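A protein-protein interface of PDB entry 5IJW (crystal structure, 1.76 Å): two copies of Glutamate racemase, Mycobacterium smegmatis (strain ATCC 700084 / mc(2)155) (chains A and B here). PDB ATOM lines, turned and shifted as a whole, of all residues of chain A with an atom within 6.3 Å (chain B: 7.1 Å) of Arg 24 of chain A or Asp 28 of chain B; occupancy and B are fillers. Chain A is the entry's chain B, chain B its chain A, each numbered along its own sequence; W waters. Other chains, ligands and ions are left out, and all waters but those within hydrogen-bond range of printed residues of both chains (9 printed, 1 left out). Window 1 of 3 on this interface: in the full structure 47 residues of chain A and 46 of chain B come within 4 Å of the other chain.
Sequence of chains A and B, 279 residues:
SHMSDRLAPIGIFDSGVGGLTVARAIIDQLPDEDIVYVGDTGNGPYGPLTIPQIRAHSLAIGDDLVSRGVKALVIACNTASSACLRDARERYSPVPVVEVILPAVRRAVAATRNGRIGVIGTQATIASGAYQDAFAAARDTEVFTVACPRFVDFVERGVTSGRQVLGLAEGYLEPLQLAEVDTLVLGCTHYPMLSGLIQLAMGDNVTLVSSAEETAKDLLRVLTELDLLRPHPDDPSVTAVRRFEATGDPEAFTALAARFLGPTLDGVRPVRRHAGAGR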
ATOM      1  N   GLY A  19      -8.911 -12.112  41.079  1.00  0.00           N
ATOM      2  CA  GLY A  19      -9.532 -13.362  40.671  1.00  0.00           C
ATOM      3  C   GLY A  19     -10.709 -13.191  39.741  1.00  0.00           C
ATOM      4  O   GLY A  19     -11.177 -14.183  39.169  1.00  0.00           O
ATOM      5  N   LEU A  20     -11.196 -11.961  39.566  1.00  0.00           N
ATOM      6  CA  LEU A  20     -12.233 -11.727  38.576  1.00  0.00           C
ATOM      7  C   LEU A  20     -11.756 -12.039  37.158  1.00  0.00           C
ATOM      8  O   LEU A  20     -12.597 -12.238  36.280  1.00  0.00           O
ATOM      9  CB  LEU A  20     -12.740 -10.284  38.683  1.00  0.00           C
ATOM     10  CG  LEU A  20     -13.599  -9.957  39.912  1.00  0.00           C
ATOM     11  CD1 LEU A  20     -14.002  -8.468  39.912  1.00  0.00           C
ATOM     12  CD2 LEU A  20     -14.858 -10.829  40.000  1.00  0.00           C
ATOM     13  N   THR A  21     -10.437 -12.097  36.898  1.00  0.00           N
ATOM     14  CA  THR A  21     -10.007 -12.578  35.582  1.00  0.00           C
ATOM     15  C   THR A  21     -10.415 -14.033  35.398  1.00  0.00           C
ATOM     16  O   THR A  21     -10.846 -14.430  34.309  1.00  0.00           O
ATOM     17  CB  THR A  21      -8.492 -12.428  35.354  1.00  0.00           C
ATOM     18  OG1 THR A  21      -7.750 -13.272  36.254  1.00  0.00           O
ATOM     19  CG2 THR A  21      -8.047 -10.962  35.486  1.00  0.00           C
ATOM     20  N   VAL A  22     -10.314 -14.831  36.463  1.00  0.00           N
ATOM     21  CA  VAL A  22     -10.751 -16.220  36.390  1.00  0.00           C
ATOM     22  C   VAL A  22     -12.271 -16.300  36.344  1.00  0.00           C
ATOM     23  O   VAL A  22     -12.837 -17.055  35.548  1.00  0.00           O
ATOM     24  CB  VAL A  22     -10.166 -17.024  37.563  1.00  0.00           C
ATOM     25  CG1 VAL A  22     -10.565 -18.503  37.453  1.00  0.00           C
ATOM     26  CG2 VAL A  22      -8.652 -16.868  37.577  1.00  0.00           C
ATOM     27  N   ALA A  23     -12.958 -15.510  37.172  1.00  0.00           N
ATOM     28  CA  ALA A  23     -14.419 -15.525  37.148  1.00  0.00           C
ATOM     29  C   ALA A  23     -14.963 -15.110  35.783  1.00  0.00           C
ATOM     30  O   ALA A  23     -15.915 -15.724  35.274  1.00  0.00           O
ATOM     31  CB  ALA A  23     -14.976 -14.616  38.244  1.00  0.00           C
ATOM     32  N   ARG A  24     -14.368 -14.078  35.170  1.00  0.00           N
ATOM     33  CA  ARG A  24     -14.861 -13.605  33.881  1.00  0.00           C
ATOM     34  C   ARG A  24     -14.676 -14.668  32.806  1.00  0.00           C
ATOM     35  O   ARG A  24     -15.568 -14.889  31.981  1.00  0.00           O
ATOM     36  CB  ARG A  24     -14.153 -12.308  33.486  1.00  0.00           C
ATOM     37  CG  ARG A  24     -14.898 -11.465  32.460  1.00  0.00           C
ATOM     38  CD  ARG A  24     -14.040 -10.252  32.041  1.00  0.00           C
ATOM     39  NE  ARG A  24     -13.025 -10.634  31.063  1.00  0.00           N
ATOM     40  CZ  ARG A  24     -12.094  -9.819  30.568  1.00  0.00           C
ATOM     41  NH1 ARG A  24     -12.014  -8.550  30.971  1.00  0.00           N
ATOM     42  NH2 ARG A  24     -11.245 -10.278  29.655  1.00  0.00           N
ATOM     43  N   ALA A  25     -13.528 -15.344  32.808  1.00  0.00           N
ATOM     44  CA  ALA A  25     -13.297 -16.426  31.851  1.00  0.00           C
ATOM     45  C   ALA A  25     -14.249 -17.595  32.078  1.00  0.00           C
ATOM     46  O   ALA A  25     -14.717 -18.219  31.113  1.00  0.00           O
ATOM     47  CB  ALA A  25     -11.842 -16.898  31.943  1.00  0.00           C
ATOM     48  N   ILE A  26     -14.544 -17.916  33.339  1.00  0.00           N
ATOM     49  CA  ILE A  26     -15.515 -18.971  33.635  1.00  0.00           C
ATOM     50  C   ILE A  26     -16.898 -18.590  33.116  1.00  0.00           C
ATOM     51  O   ILE A  26     -17.587 -19.395  32.479  1.00  0.00           O
ATOM     52  CB  ILE A  26     -15.540 -19.252  35.148  1.00  0.00           C
ATOM     53  CG1 ILE A  26     -14.249 -19.976  35.556  1.00  0.00           C
ATOM     54  CG2 ILE A  26     -16.801 -20.042  35.557  1.00  0.00           C
ATOM     55  CD1 ILE A  26     -14.039 -20.086  37.078  1.00  0.00           C
ATOM     56  N   ILE A  27     -17.333 -17.358  33.389  1.00  0.00           N
ATOM     57  CA  ILE A  27     -18.653 -16.925  32.938  1.00  0.00           C
ATOM     58  C   ILE A  27     -18.731 -16.938  31.413  1.00  0.00           C
ATOM     59  O   ILE A  27     -19.775 -17.277  30.833  1.00  0.00           O
ATOM     60  CB  ILE A  27     -18.968 -15.542  33.541  1.00  0.00           C
ATOM     61  CG1 ILE A  27     -19.113 -15.686  35.066  1.00  0.00           C
ATOM     62  CG2 ILE A  27     -20.205 -14.927  32.896  1.00  0.00           C
ATOM     63  CD1 ILE A  27     -19.067 -14.370  35.824  1.00  0.00           C
ATOM     64  N   ASP A  28     -17.626 -16.597  30.742  1.00  0.00           N
ATOM     65  CA  ASP A  28     -17.572 -16.692  29.281  1.00  0.00           C
ATOM     66  C   ASP A  28     -17.908 -18.101  28.814  1.00  0.00           C
ATOM     67  O   ASP A  28     -18.660 -18.286  27.848  1.00  0.00           O
ATOM     68  CB  ASP A  28     -16.182 -16.330  28.757  1.00  0.00           C
ATOM     69  CG  ASP A  28     -15.915 -14.833  28.714  1.00  0.00           C
ATOM     70  OD1 ASP A  28     -16.854 -14.004  28.785  1.00  0.00           O
ATOM     71  OD2 ASP A  28     -14.726 -14.494  28.583  1.00  0.00           O
ATOM     72  N   GLN A  29     -17.311 -19.109  29.459  1.00  0.00           N
ATOM     73  CA  GLN A  29     -17.484 -20.482  29.001  1.00  0.00           C
ATOM     74  C   GLN A  29     -18.805 -21.073  29.468  1.00  0.00           C
ATOM     75  O   GLN A  29     -19.348 -21.967  28.810  1.00  0.00           O
ATOM     76  CB  GLN A  29     -16.332 -21.357  29.506  1.00  0.00           C
ATOM     77  CG  GLN A  29     -14.963 -20.936  28.994  1.00  0.00           C
ATOM     78  CD  GLN A  29     -14.907 -20.893  27.478  1.00  0.00           C
ATOM     79  OE1 GLN A  29     -15.335 -21.837  26.807  1.00  0.00           O
ATOM     80  NE2 GLN A  29     -14.383 -19.791  26.925  1.00  0.00           N
ATOM     81  N   THR A 160       0.243  -0.797  32.423  1.00  0.00           N
ATOM     82  CA  THR A 160       0.539  -2.090  31.816  1.00  0.00           C
ATOM     83  C   THR A 160       1.132  -1.928  30.419  1.00  0.00           C
ATOM     84  O   THR A 160       1.091  -2.864  29.614  1.00  0.00           O
ATOM     85  CB  THR A 160      -0.722  -2.953  31.776  1.00  0.00           C
ATOM     86  OG1 THR A 160      -1.777  -2.227  31.131  1.00  0.00           O
ATOM     87  CG2 THR A 160      -1.172  -3.331  33.197  1.00  0.00           C
ATOM     88  N   PRO A 192      -2.855 -11.707  33.208  1.00  0.00           N
ATOM     89  CA  PRO A 192      -3.483 -11.528  31.884  1.00  0.00           C
ATOM     90  C   PRO A 192      -3.501 -10.080  31.423  1.00  0.00           C
ATOM     91  O   PRO A 192      -3.417  -9.822  30.217  1.00  0.00           O
ATOM     92  CB  PRO A 192      -4.900 -12.063  32.096  1.00  0.00           C
ATOM     93  CG  PRO A 192      -4.739 -13.108  33.135  1.00  0.00           C
ATOM     94  CD  PRO A 192      -3.710 -12.542  34.081  1.00  0.00           C
ATOM     95  N   MET A 193      -3.606  -9.122  32.352  1.00  0.00           N
ATOM     96  CA  MET A 193      -3.585  -7.711  31.979  1.00  0.00           C
ATOM     97  C   MET A 193      -2.203  -7.234  31.539  1.00  0.00           C
ATOM     98  O   MET A 193      -2.083  -6.110  31.030  1.00  0.00           O
ATOM     99  CB  MET A 193      -4.064  -6.842  33.146  1.00  0.00           C
ATOM    100  CG  MET A 193      -5.101  -7.477  34.060  1.00  0.00           C
ATOM    101  SD  MET A 193      -6.600  -7.988  33.238  1.00  0.00           S
ATOM    102  CE  MET A 193      -7.216  -6.417  32.647  1.00  0.00           C
ATOM    103  N   LEU A 194      -1.161  -8.037  31.740  1.00  0.00           N
ATOM    104  CA  LEU A 194       0.192  -7.693  31.320  1.00  0.00           C
ATOM    105  C   LEU A 194       0.652  -8.523  30.133  1.00  0.00           C
ATOM    106  O   LEU A 194       1.832  -8.476  29.784  1.00  0.00           O
ATOM    107  CB  LEU A 194       1.184  -7.881  32.478  1.00  0.00           C
ATOM    108  CG  LEU A 194       1.332  -6.729  33.464  1.00  0.00           C
ATOM    109  CD1 LEU A 194       2.201  -7.172  34.655  1.00  0.00           C
ATOM    110  CD2 LEU A 194       1.941  -5.509  32.769  1.00  0.00           C
ATOM    111  N   ARG A 259     -11.014  -2.641  36.833  1.00  0.00           N
ATOM    112  CA  ARG A 259      -9.782  -3.054  36.168  1.00  0.00           C
ATOM    113  C   ARG A 259      -9.938  -4.409  35.485  1.00  0.00           C
ATOM    114  O   ARG A 259      -9.318  -4.657  34.444  1.00  0.00           O
ATOM    115  CB  ARG A 259      -8.636  -3.114  37.179  1.00  0.00           C
ATOM    116  CG  ARG A 259      -8.268  -1.764  37.811  1.00  0.00           C
ATOM    117  CD  ARG A 259      -7.475  -0.895  36.843  1.00  0.00           C
ATOM    118  NE  ARG A 259      -6.340  -1.641  36.300  1.00  0.00           N
ATOM    119  CZ  ARG A 259      -6.218  -2.021  35.030  1.00  0.00           C
ATOM    120  NH1 ARG A 259      -7.150  -1.691  34.145  1.00  0.00           N
ATOM    121  NH2 ARG A 259      -5.148  -2.713  34.643  1.00  0.00           N
ATOM    122  N   PHE A 260     -10.764  -5.298  36.045  1.00  0.00           N
ATOM    123  CA  PHE A 260     -10.806  -6.678  35.581  1.00  0.00           C
ATOM    124  C   PHE A 260     -12.082  -7.050  34.835  1.00  0.00           C
ATOM    125  O   PHE A 260     -12.049  -7.980  34.024  1.00  0.00           O
ATOM    126  CB  PHE A 260     -10.592  -7.632  36.771  1.00  0.00           C
ATOM    127  CG  PHE A 260      -9.337  -7.333  37.547  1.00  0.00           C
ATOM    128  CD1 PHE A 260      -8.096  -7.733  37.063  1.00  0.00           C
ATOM    129  CD2 PHE A 260      -9.388  -6.626  38.746  1.00  0.00           C
ATOM    130  CE1 PHE A 260      -6.928  -7.443  37.761  1.00  0.00           C
ATOM    131  CE2 PHE A 260      -8.220  -6.338  39.449  1.00  0.00           C
ATOM    132  CZ  PHE A 260      -6.994  -6.736  38.955  1.00  0.00           C
ATOM    133  N   LEU A 261     -13.182  -6.342  35.049  1.00  0.00           N
ATOM    134  CA  LEU A 261     -14.412  -6.664  34.340  1.00  0.00           C
ATOM    135  C   LEU A 261     -14.462  -5.938  32.995  1.00  0.00           C
ATOM    136  O   LEU A 261     -13.730  -4.974  32.750  1.00  0.00           O
ATOM    137  CB  LEU A 261     -15.635  -6.298  35.184  1.00  0.00           C
ATOM    138  CG  LEU A 261     -15.779  -7.077  36.497  1.00  0.00           C
ATOM    139  CD1 LEU A 261     -16.984  -6.582  37.297  1.00  0.00           C
ATOM    140  CD2 LEU A 261     -15.891  -8.567  36.239  1.00  0.00           C
ATOM    141  N   GLY A 262     -15.332  -6.429  32.112  1.00  0.00           N
ATOM    142  CA  GLY A 262     -15.550  -5.803  30.826  1.00  0.00           C
ATOM    143  C   GLY A 262     -16.043  -4.375  30.967  1.00  0.00           C
ATOM    144  O   GLY A 262     -16.601  -3.986  31.998  1.00  0.00           O
ATOM    145  N   PRO A 263     -15.851  -3.565  29.930  1.00  0.00           N
ATOM    146  CA  PRO A 263     -16.279  -2.168  30.011  1.00  0.00           C
ATOM    147  C   PRO A 263     -17.792  -2.075  30.064  1.00  0.00           C
ATOM    148  O   PRO A 263     -18.509  -2.963  29.597  1.00  0.00           O
ATOM    149  CB  PRO A 263     -15.728  -1.554  28.720  1.00  0.00           C
ATOM    150  CG  PRO A 263     -15.757  -2.697  27.754  1.00  0.00           C
ATOM    151  CD  PRO A 263     -15.406  -3.924  28.570  1.00  0.00           C
ATOM    152  N   THR B  21     -15.326  -9.183  21.871  1.00  0.00           N
ATOM    153  CA  THR B  21     -14.250 -10.006  22.430  1.00  0.00           C
ATOM    154  C   THR B  21     -12.895  -9.373  22.154  1.00  0.00           C
ATOM    155  O   THR B  21     -12.000  -9.397  23.012  1.00  0.00           O
ATOM    156  CB  THR B  21     -14.282 -11.433  21.863  1.00  0.00           C
ATOM    157  OG1 THR B  21     -13.952 -11.413  20.465  1.00  0.00           O
ATOM    158  CG2 THR B  21     -15.650 -12.079  22.070  1.00  0.00           C
ATOM    159  N   VAL B  22     -12.726  -8.809  20.957  1.00  0.00           N
ATOM    160  CA  VAL B  22     -11.486  -8.120  20.612  1.00  0.00           C
ATOM    161  C   VAL B  22     -11.382  -6.797  21.363  1.00  0.00           C
ATOM    162  O   VAL B  22     -10.320  -6.451  21.895  1.00  0.00           O
ATOM    163  CB  VAL B  22     -11.405  -7.910  19.088  1.00  0.00           C
ATOM    164  CG1 VAL B  22     -10.132  -7.169  18.727  1.00  0.00           C
ATOM    165  CG2 VAL B  22     -11.484  -9.256  18.346  1.00  0.00           C
ATOM    166  N   ALA B  23     -12.473  -6.026  21.406  1.00  0.00           N
ATOM    167  CA  ALA B  23     -12.426  -4.760  22.125  1.00  0.00           C
ATOM    168  C   ALA B  23     -12.121  -4.995  23.597  1.00  0.00           C
ATOM    169  O   ALA B  23     -11.303  -4.286  24.192  1.00  0.00           O
ATOM    170  CB  ALA B  23     -13.743  -4.000  21.958  1.00  0.00           C
ATOM    171  N   ARG B  24     -12.748  -6.015  24.191  1.00  0.00           N
ATOM    172  CA  ARG B  24     -12.485  -6.308  25.595  1.00  0.00           C
ATOM    173  C   ARG B  24     -11.017  -6.653  25.817  1.00  0.00           C
ATOM    174  O   ARG B  24     -10.390  -6.154  26.761  1.00  0.00           O
ATOM    175  CB  ARG B  24     -13.387  -7.442  26.083  1.00  0.00           C
ATOM    176  CG  ARG B  24     -13.358  -7.619  27.599  1.00  0.00           C
ATOM    177  CD  ARG B  24     -14.285  -8.742  28.077  1.00  0.00           C
ATOM    178  NE  ARG B  24     -13.966 -10.024  27.451  1.00  0.00           N
ATOM    179  CZ  ARG B  24     -14.602 -11.167  27.709  1.00  0.00           C
ATOM    180  NH1 ARG B  24     -15.600 -11.190  28.584  1.00  0.00           N
ATOM    181  NH2 ARG B  24     -14.253 -12.285  27.079  1.00  0.00           N
ATOM    182  N   ALA B  25     -10.445  -7.487  24.947  1.00  0.00           N
ATOM    183  CA  ALA B  25      -9.035  -7.843  25.096  1.00  0.00           C
ATOM    184  C   ALA B  25      -8.127  -6.632  24.914  1.00  0.00           C
ATOM    185  O   ALA B  25      -7.084  -6.528  25.565  1.00  0.00           O
ATOM    186  CB  ALA B  25      -8.664  -8.935  24.089  1.00  0.00           C
ATOM    187  N   ILE B  26      -8.476  -5.730  23.997  1.00  0.00           N
ATOM    188  CA  ILE B  26      -7.693  -4.508  23.823  1.00  0.00           C
ATOM    189  C   ILE B  26      -7.764  -3.655  25.082  1.00  0.00           C
ATOM    190  O   ILE B  26      -6.746  -3.168  25.582  1.00  0.00           O
ATOM    191  CB  ILE B  26      -8.185  -3.734  22.586  1.00  0.00           C
ATOM    192  CG1 ILE B  26      -7.661  -4.404  21.310  1.00  0.00           C
ATOM    193  CG2 ILE B  26      -7.788  -2.266  22.654  1.00  0.00           C
ATOM    194  CD1 ILE B  26      -8.397  -3.967  20.047  1.00  0.00           C
ATOM    195  N   ILE B  27      -8.970  -3.487  25.624  1.00  0.00           N
ATOM    196  CA  ILE B  27      -9.131  -2.657  26.809  1.00  0.00           C
ATOM    197  C   ILE B  27      -8.408  -3.274  28.005  1.00  0.00           C
ATOM    198  O   ILE B  27      -7.859  -2.550  28.851  1.00  0.00           O
ATOM    199  CB  ILE B  27     -10.633  -2.438  27.064  1.00  0.00           C
ATOM    200  CG1 ILE B  27     -11.213  -1.541  25.965  1.00  0.00           C
ATOM    201  CG2 ILE B  27     -10.883  -1.855  28.459  1.00  0.00           C
ATOM    202  CD1 ILE B  27     -12.729  -1.613  25.837  1.00  0.00           C
ATOM    203  N   ASP B  28      -8.381  -4.611  28.088  1.00  0.00           N
ATOM    204  CA  ASP B  28      -7.607  -5.281  29.134  1.00  0.00           C
ATOM    205  C   ASP B  28      -6.149  -4.848  29.097  1.00  0.00           C
ATOM    206  O   ASP B  28      -5.528  -4.639  30.148  1.00  0.00           O
ATOM    207  CB  ASP B  28      -7.654  -6.805  28.970  1.00  0.00           C
ATOM    208  CG  ASP B  28      -8.979  -7.423  29.380  1.00  0.00           C
ATOM    209  OD1 ASP B  28      -9.806  -6.772  30.055  1.00  0.00           O
ATOM    210  OD2 ASP B  28      -9.176  -8.600  29.016  1.00  0.00           O
ATOM    211  N   GLN B  29      -5.575  -4.757  27.889  1.00  0.00           N
ATOM    212  CA  GLN B  29      -4.164  -4.415  27.738  1.00  0.00           C
ATOM    213  C   GLN B  29      -3.918  -2.920  27.811  1.00  0.00           C
ATOM    214  O   GLN B  29      -2.826  -2.503  28.209  1.00  0.00           O
ATOM    215  CB  GLN B  29      -3.633  -4.914  26.391  1.00  0.00           C
ATOM    216  CG  GLN B  29      -3.766  -6.405  26.205  1.00  0.00           C
ATOM    217  CD  GLN B  29      -3.071  -7.164  27.308  1.00  0.00           C
ATOM    218  OE1 GLN B  29      -1.910  -6.884  27.640  1.00  0.00           O
ATOM    219  NE2 GLN B  29      -3.773  -8.120  27.896  1.00  0.00           N
ATOM    220  N   LEU B  30      -4.893  -2.111  27.395  1.00  0.00           N
ATOM    221  CA  LEU B  30      -4.679  -0.687  27.125  1.00  0.00           C
ATOM    222  C   LEU B  30      -5.784   0.122  27.798  1.00  0.00           C
ATOM    223  O   LEU B  30      -6.617   0.747  27.129  1.00  0.00           O
ATOM    224  CB  LEU B  30      -4.633  -0.435  25.615  1.00  0.00           C
ATOM    225  CG  LEU B  30      -3.431  -1.050  24.886  1.00  0.00           C
ATOM    226  CD1 LEU B  30      -3.743  -1.252  23.400  1.00  0.00           C
ATOM    227  CD2 LEU B  30      -2.170  -0.196  25.068  1.00  0.00           C
ATOM    228  N   PRO B  31      -5.814   0.130  29.136  1.00  0.00           N
ATOM    229  CA  PRO B  31      -6.930   0.772  29.854  1.00  0.00           C
ATOM    230  C   PRO B  31      -7.023   2.275  29.670  1.00  0.00           C
ATOM    231  O   PRO B  31      -8.102   2.836  29.901  1.00  0.00           O
ATOM    232  CB  PRO B  31      -6.642   0.440  31.323  1.00  0.00           C
ATOM    233  CG  PRO B  31      -5.163   0.165  31.359  1.00  0.00           C
ATOM    234  CD  PRO B  31      -4.859  -0.505  30.058  1.00  0.00           C
ATOM    235  N   GLU B 213      -6.898 -12.230  21.524  1.00  0.00           N
ATOM    236  CA  GLU B 213      -5.743 -12.082  22.401  1.00  0.00           C
ATOM    237  C   GLU B 213      -4.501 -11.692  21.611  1.00  0.00           C
ATOM    238  O   GLU B 213      -3.765 -10.775  22.000  1.00  0.00           O
ATOM    239  CB  GLU B 213      -5.518 -13.377  23.184  1.00  0.00           C
ATOM    240  CG  GLU B 213      -4.246 -13.399  24.045  1.00  0.00           C
ATOM    241  CD  GLU B 213      -4.257 -12.419  25.219  1.00  0.00           C
ATOM    242  OE1 GLU B 213      -5.300 -11.761  25.485  1.00  0.00           O
ATOM    243  OE2 GLU B 213      -3.193 -12.302  25.871  1.00  0.00           O
ATOM    244  N   ALA B 216      -4.899  -8.007  20.438  1.00  0.00           N
ATOM    245  CA  ALA B 216      -4.721  -7.030  21.512  1.00  0.00           C
ATOM    246  C   ALA B 216      -3.246  -6.807  21.815  1.00  0.00           C
ATOM    247  O   ALA B 216      -2.805  -5.663  21.995  1.00  0.00           O
ATOM    248  CB  ALA B 216      -5.451  -7.478  22.781  1.00  0.00           C
ATOM    249  N   ARG B 242     -14.917   5.815  26.072  1.00  0.00           N
ATOM    250  CA  ARG B 242     -15.188   4.685  25.189  1.00  0.00           C
ATOM    251  C   ARG B 242     -16.599   4.817  24.645  1.00  0.00           C
ATOM    252  O   ARG B 242     -17.556   4.946  25.417  1.00  0.00           O
ATOM    253  CB  ARG B 242     -15.014   3.350  25.923  1.00  0.00           C
ATOM    254  CG  ARG B 242     -13.646   3.190  26.566  1.00  0.00           C
ATOM    255  CD  ARG B 242     -13.412   1.776  27.086  1.00  0.00           C
ATOM    256  NE  ARG B 242     -12.131   1.699  27.783  1.00  0.00           N
ATOM    257  CZ  ARG B 242     -11.992   1.633  29.105  1.00  0.00           C
ATOM    258  NH1 ARG B 242     -13.062   1.599  29.896  1.00  0.00           N
ATOM    259  NH2 ARG B 242     -10.780   1.586  29.643  1.00  0.00           N
ATOM    260  N   PHE B 260     -20.901 -11.115  25.348  1.00  0.00           N
ATOM    261  CA  PHE B 260     -19.478 -11.028  25.056  1.00  0.00           C
ATOM    262  C   PHE B 260     -18.696 -10.231  26.081  1.00  0.00           C
ATOM    263  O   PHE B 260     -17.500 -10.478  26.255  1.00  0.00           O
ATOM    264  CB  PHE B 260     -19.275 -10.417  23.668  1.00  0.00           C
ATOM    265  CG  PHE B 260     -19.918 -11.216  22.596  1.00  0.00           C
ATOM    266  CD1 PHE B 260     -19.273 -12.322  22.069  1.00  0.00           C
ATOM    267  CD2 PHE B 260     -21.201 -10.917  22.160  1.00  0.00           C
ATOM    268  CE1 PHE B 260     -19.881 -13.098  21.092  1.00  0.00           C
ATOM    269  CE2 PHE B 260     -21.804 -11.682  21.193  1.00  0.00           C
ATOM    270  CZ  PHE B 260     -21.142 -12.778  20.658  1.00  0.00           C
ATOM    271  N   LEU B 261     -19.333  -9.290  26.767  1.00  0.00           N
ATOM    272  CA  LEU B 261     -18.598  -8.491  27.735  1.00  0.00           C
ATOM    273  C   LEU B 261     -18.537  -9.137  29.108  1.00  0.00           C
ATOM    274  O   LEU B 261     -17.598  -8.868  29.864  1.00  0.00           O
ATOM    275  CB  LEU B 261     -19.220  -7.099  27.852  1.00  0.00           C
ATOM    276  CG  LEU B 261     -18.965  -6.223  26.630  1.00  0.00           C
ATOM    277  CD1 LEU B 261     -19.538  -4.840  26.846  1.00  0.00           C
ATOM    278  CD2 LEU B 261     -17.470  -6.154  26.319  1.00  0.00           C
ATOM    279  N   GLY B 262     -19.505  -9.988  29.444  1.00  0.00           N
ATOM    280  CA  GLY B 262     -19.571 -10.564  30.766  1.00  0.00           C
ATOM    281  C   GLY B 262     -20.223  -9.598  31.725  1.00  0.00           C
ATOM    282  O   GLY B 262     -20.707  -8.536  31.323  1.00  0.00           O
ATOM    283  N   PRO B 263     -20.244  -9.935  33.015  1.00  0.00           N
ATOM    284  CA  PRO B 263     -20.865  -9.031  33.987  1.00  0.00           C
ATOM    285  C   PRO B 263     -20.036  -7.766  34.126  1.00  0.00           C
ATOM    286  O   PRO B 263     -18.807  -7.790  34.025  1.00  0.00           O
ATOM    287  CB  PRO B 263     -20.878  -9.854  35.280  1.00  0.00           C
ATOM    288  CG  PRO B 263     -19.688 -10.746  35.151  1.00  0.00           C
ATOM    289  CD  PRO B 263     -19.531 -11.048  33.670  1.00  0.00           C
HETATM  290  O   HOH W   1     -10.102  -4.635  31.650  1.00  0.00           O
HETATM  291  O   HOH W   2      -9.725 -10.932  26.698  1.00  0.00           O
HETATM  292  O   HOH W   3     -19.455 -13.357  29.044  1.00  0.00           O
HETATM  293  O   HOH W   4     -12.525 -13.252  29.926  1.00  0.00           O
HETATM  294  O   HOH W   5      -8.476  -2.510  31.412  1.00  0.00           O
HETATM  295  O   HOH W   6      -4.281  -3.299  31.929  1.00  0.00           O
HETATM  296  O   HOH W   7     -17.044  -8.628  32.591  1.00  0.00           O
HETATM  297  O   HOH W   8      -4.846 -11.531  28.381  1.00  0.00           O
HETATM  298  O   HOH W   9      -1.564  -0.021  28.773  1.00  0.00           O
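Ile 27 of chain A touches Pro 263 of chain B, and with the chains exchanged Pro 263 of chain A touches Ile 27 of chain B. Gly 262 of chain A touches Leu 261 of chain B, but with the chains exchanged Leu 261 of chain A does not touch Gly 262 of chain B (6.3 Å).
Water W9 lies within hydrogen-bond range of the backbone carbonyl oxygen (O) of Gln 29 of chain B (2.8 Å) and the side-chain hydroxyl (OG1) of Thr 160 of chain A (3.2 Å). Water W8 bridges O of Pro 192 of chain A and OE1 of Glu 213 of chain B.
Arg 24 of chain A touches two residues of chain B. Of the printed residues of chain A, Asp 28 of chain B touches Arg 24 (2.7 Å) and Met 193 (3.5 Å). Of the printed residues of chain B, Gly 262 of chain A touches Leu 261. Of the printed residues of chain A, Pro 263 of chain B touches Ile 27 and Leu 261. Of the printed residues of chain B, Leu 194 of chain A touches Gln 29. The nearest residue of chain B that does not touch Arg 24 of chain A is Leu 261 of chain B (4.4 Å).
The backbone carbonyl oxygen (O) of Leu 261 of chain B lies within hydrogen-bond range of the guanidinium group (NH1) of Arg 24 of chain B (3.3 Å). The backbone carbonyl oxygen of Phe 260 of chain B is in hydrogen-bond range of the guanidinium group of Arg 24 of chain B, 3.1 Å away.
O of Pro 192 of chain A sits at hydrogen-bond distance from NE2 of Gln 29 of chain B, 2.9 Å away. NH2 of Arg 24 of chain A lies within salt-bridge range of OD2 of Asp 28 of chain B (2.7 Å). OE1 of Gln 29 of chain B lies close to O of Met 193 of chain A (3.5 Å). The guanidinium group (NH2) of Arg 24 of chain B is in salt-bridge range of the side-chain carboxylate (OD2) of Asp 28 of chain A (2.7 Å). The side-chain hydroxyl of Thr 160 of chain A lies within hydrogen-bond range of the backbone carbonyl oxygen of Gln 29 of chain B, 3.1 Å away.
Among the printed residues, pairs that only touch across the chains: Arg 24 of chain A with Arg 24 of chain B (3.5 Å), Ile 27 of chain A with Pro 263 of chain B (3.7 Å), Thr 160 of chain A with Pro 31 of chain B (3.7 Å), Met 193 of chain A with Asp 28 of chain B (3.5 Å), Leu 194 of chain A with Gln 29 of chain B (3.9 Å), Arg 259 of chain A with Pro 31 of chain B (3.6 Å), Leu 261 of chain A with Pro 263 of chain B (3.7 Å), Gly 262 of chain A with Leu 261 of chain B (3.8 Å), Pro 263 of chain A with Ile 27 of chain B (3.7 Å) and Pro 263 of chain A with Leu 261 of chain B (3.5 Å).
Printed residues of chain A that touch a printed residue of chain B: Arg 24, Ile 27, Asp 28, Thr 160, Pro 192, Met 193, Leu 194, Arg 259, Leu 261, Gly 262 and Pro 263. Hydrophobic or aromatic side chains of chain A that line the printed part of chain B: Ile 27, Met 193, Leu 261 and Pro 263. Printed residues of chain B that touch a printed residue of chain A: Arg 24, Ile 27, Asp 28, Gln 29, Pro 31, Leu 261 and Pro 263. Hydrophobic or aromatic side chains of chain B that line the printed part of chain A: Ile 27, Pro 31, Leu 261 and Pro 263. Among the printed residues, 15 pairs touch across the chains. Among the printed residues, Asp or Glu carboxylates within 4 Å of a Lys or Arg side-chain nitrogen of the other chain: Arg 24 of chain A with Asp 28 of chain B and Asp 28 of chain A with Arg 24 of chain B.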
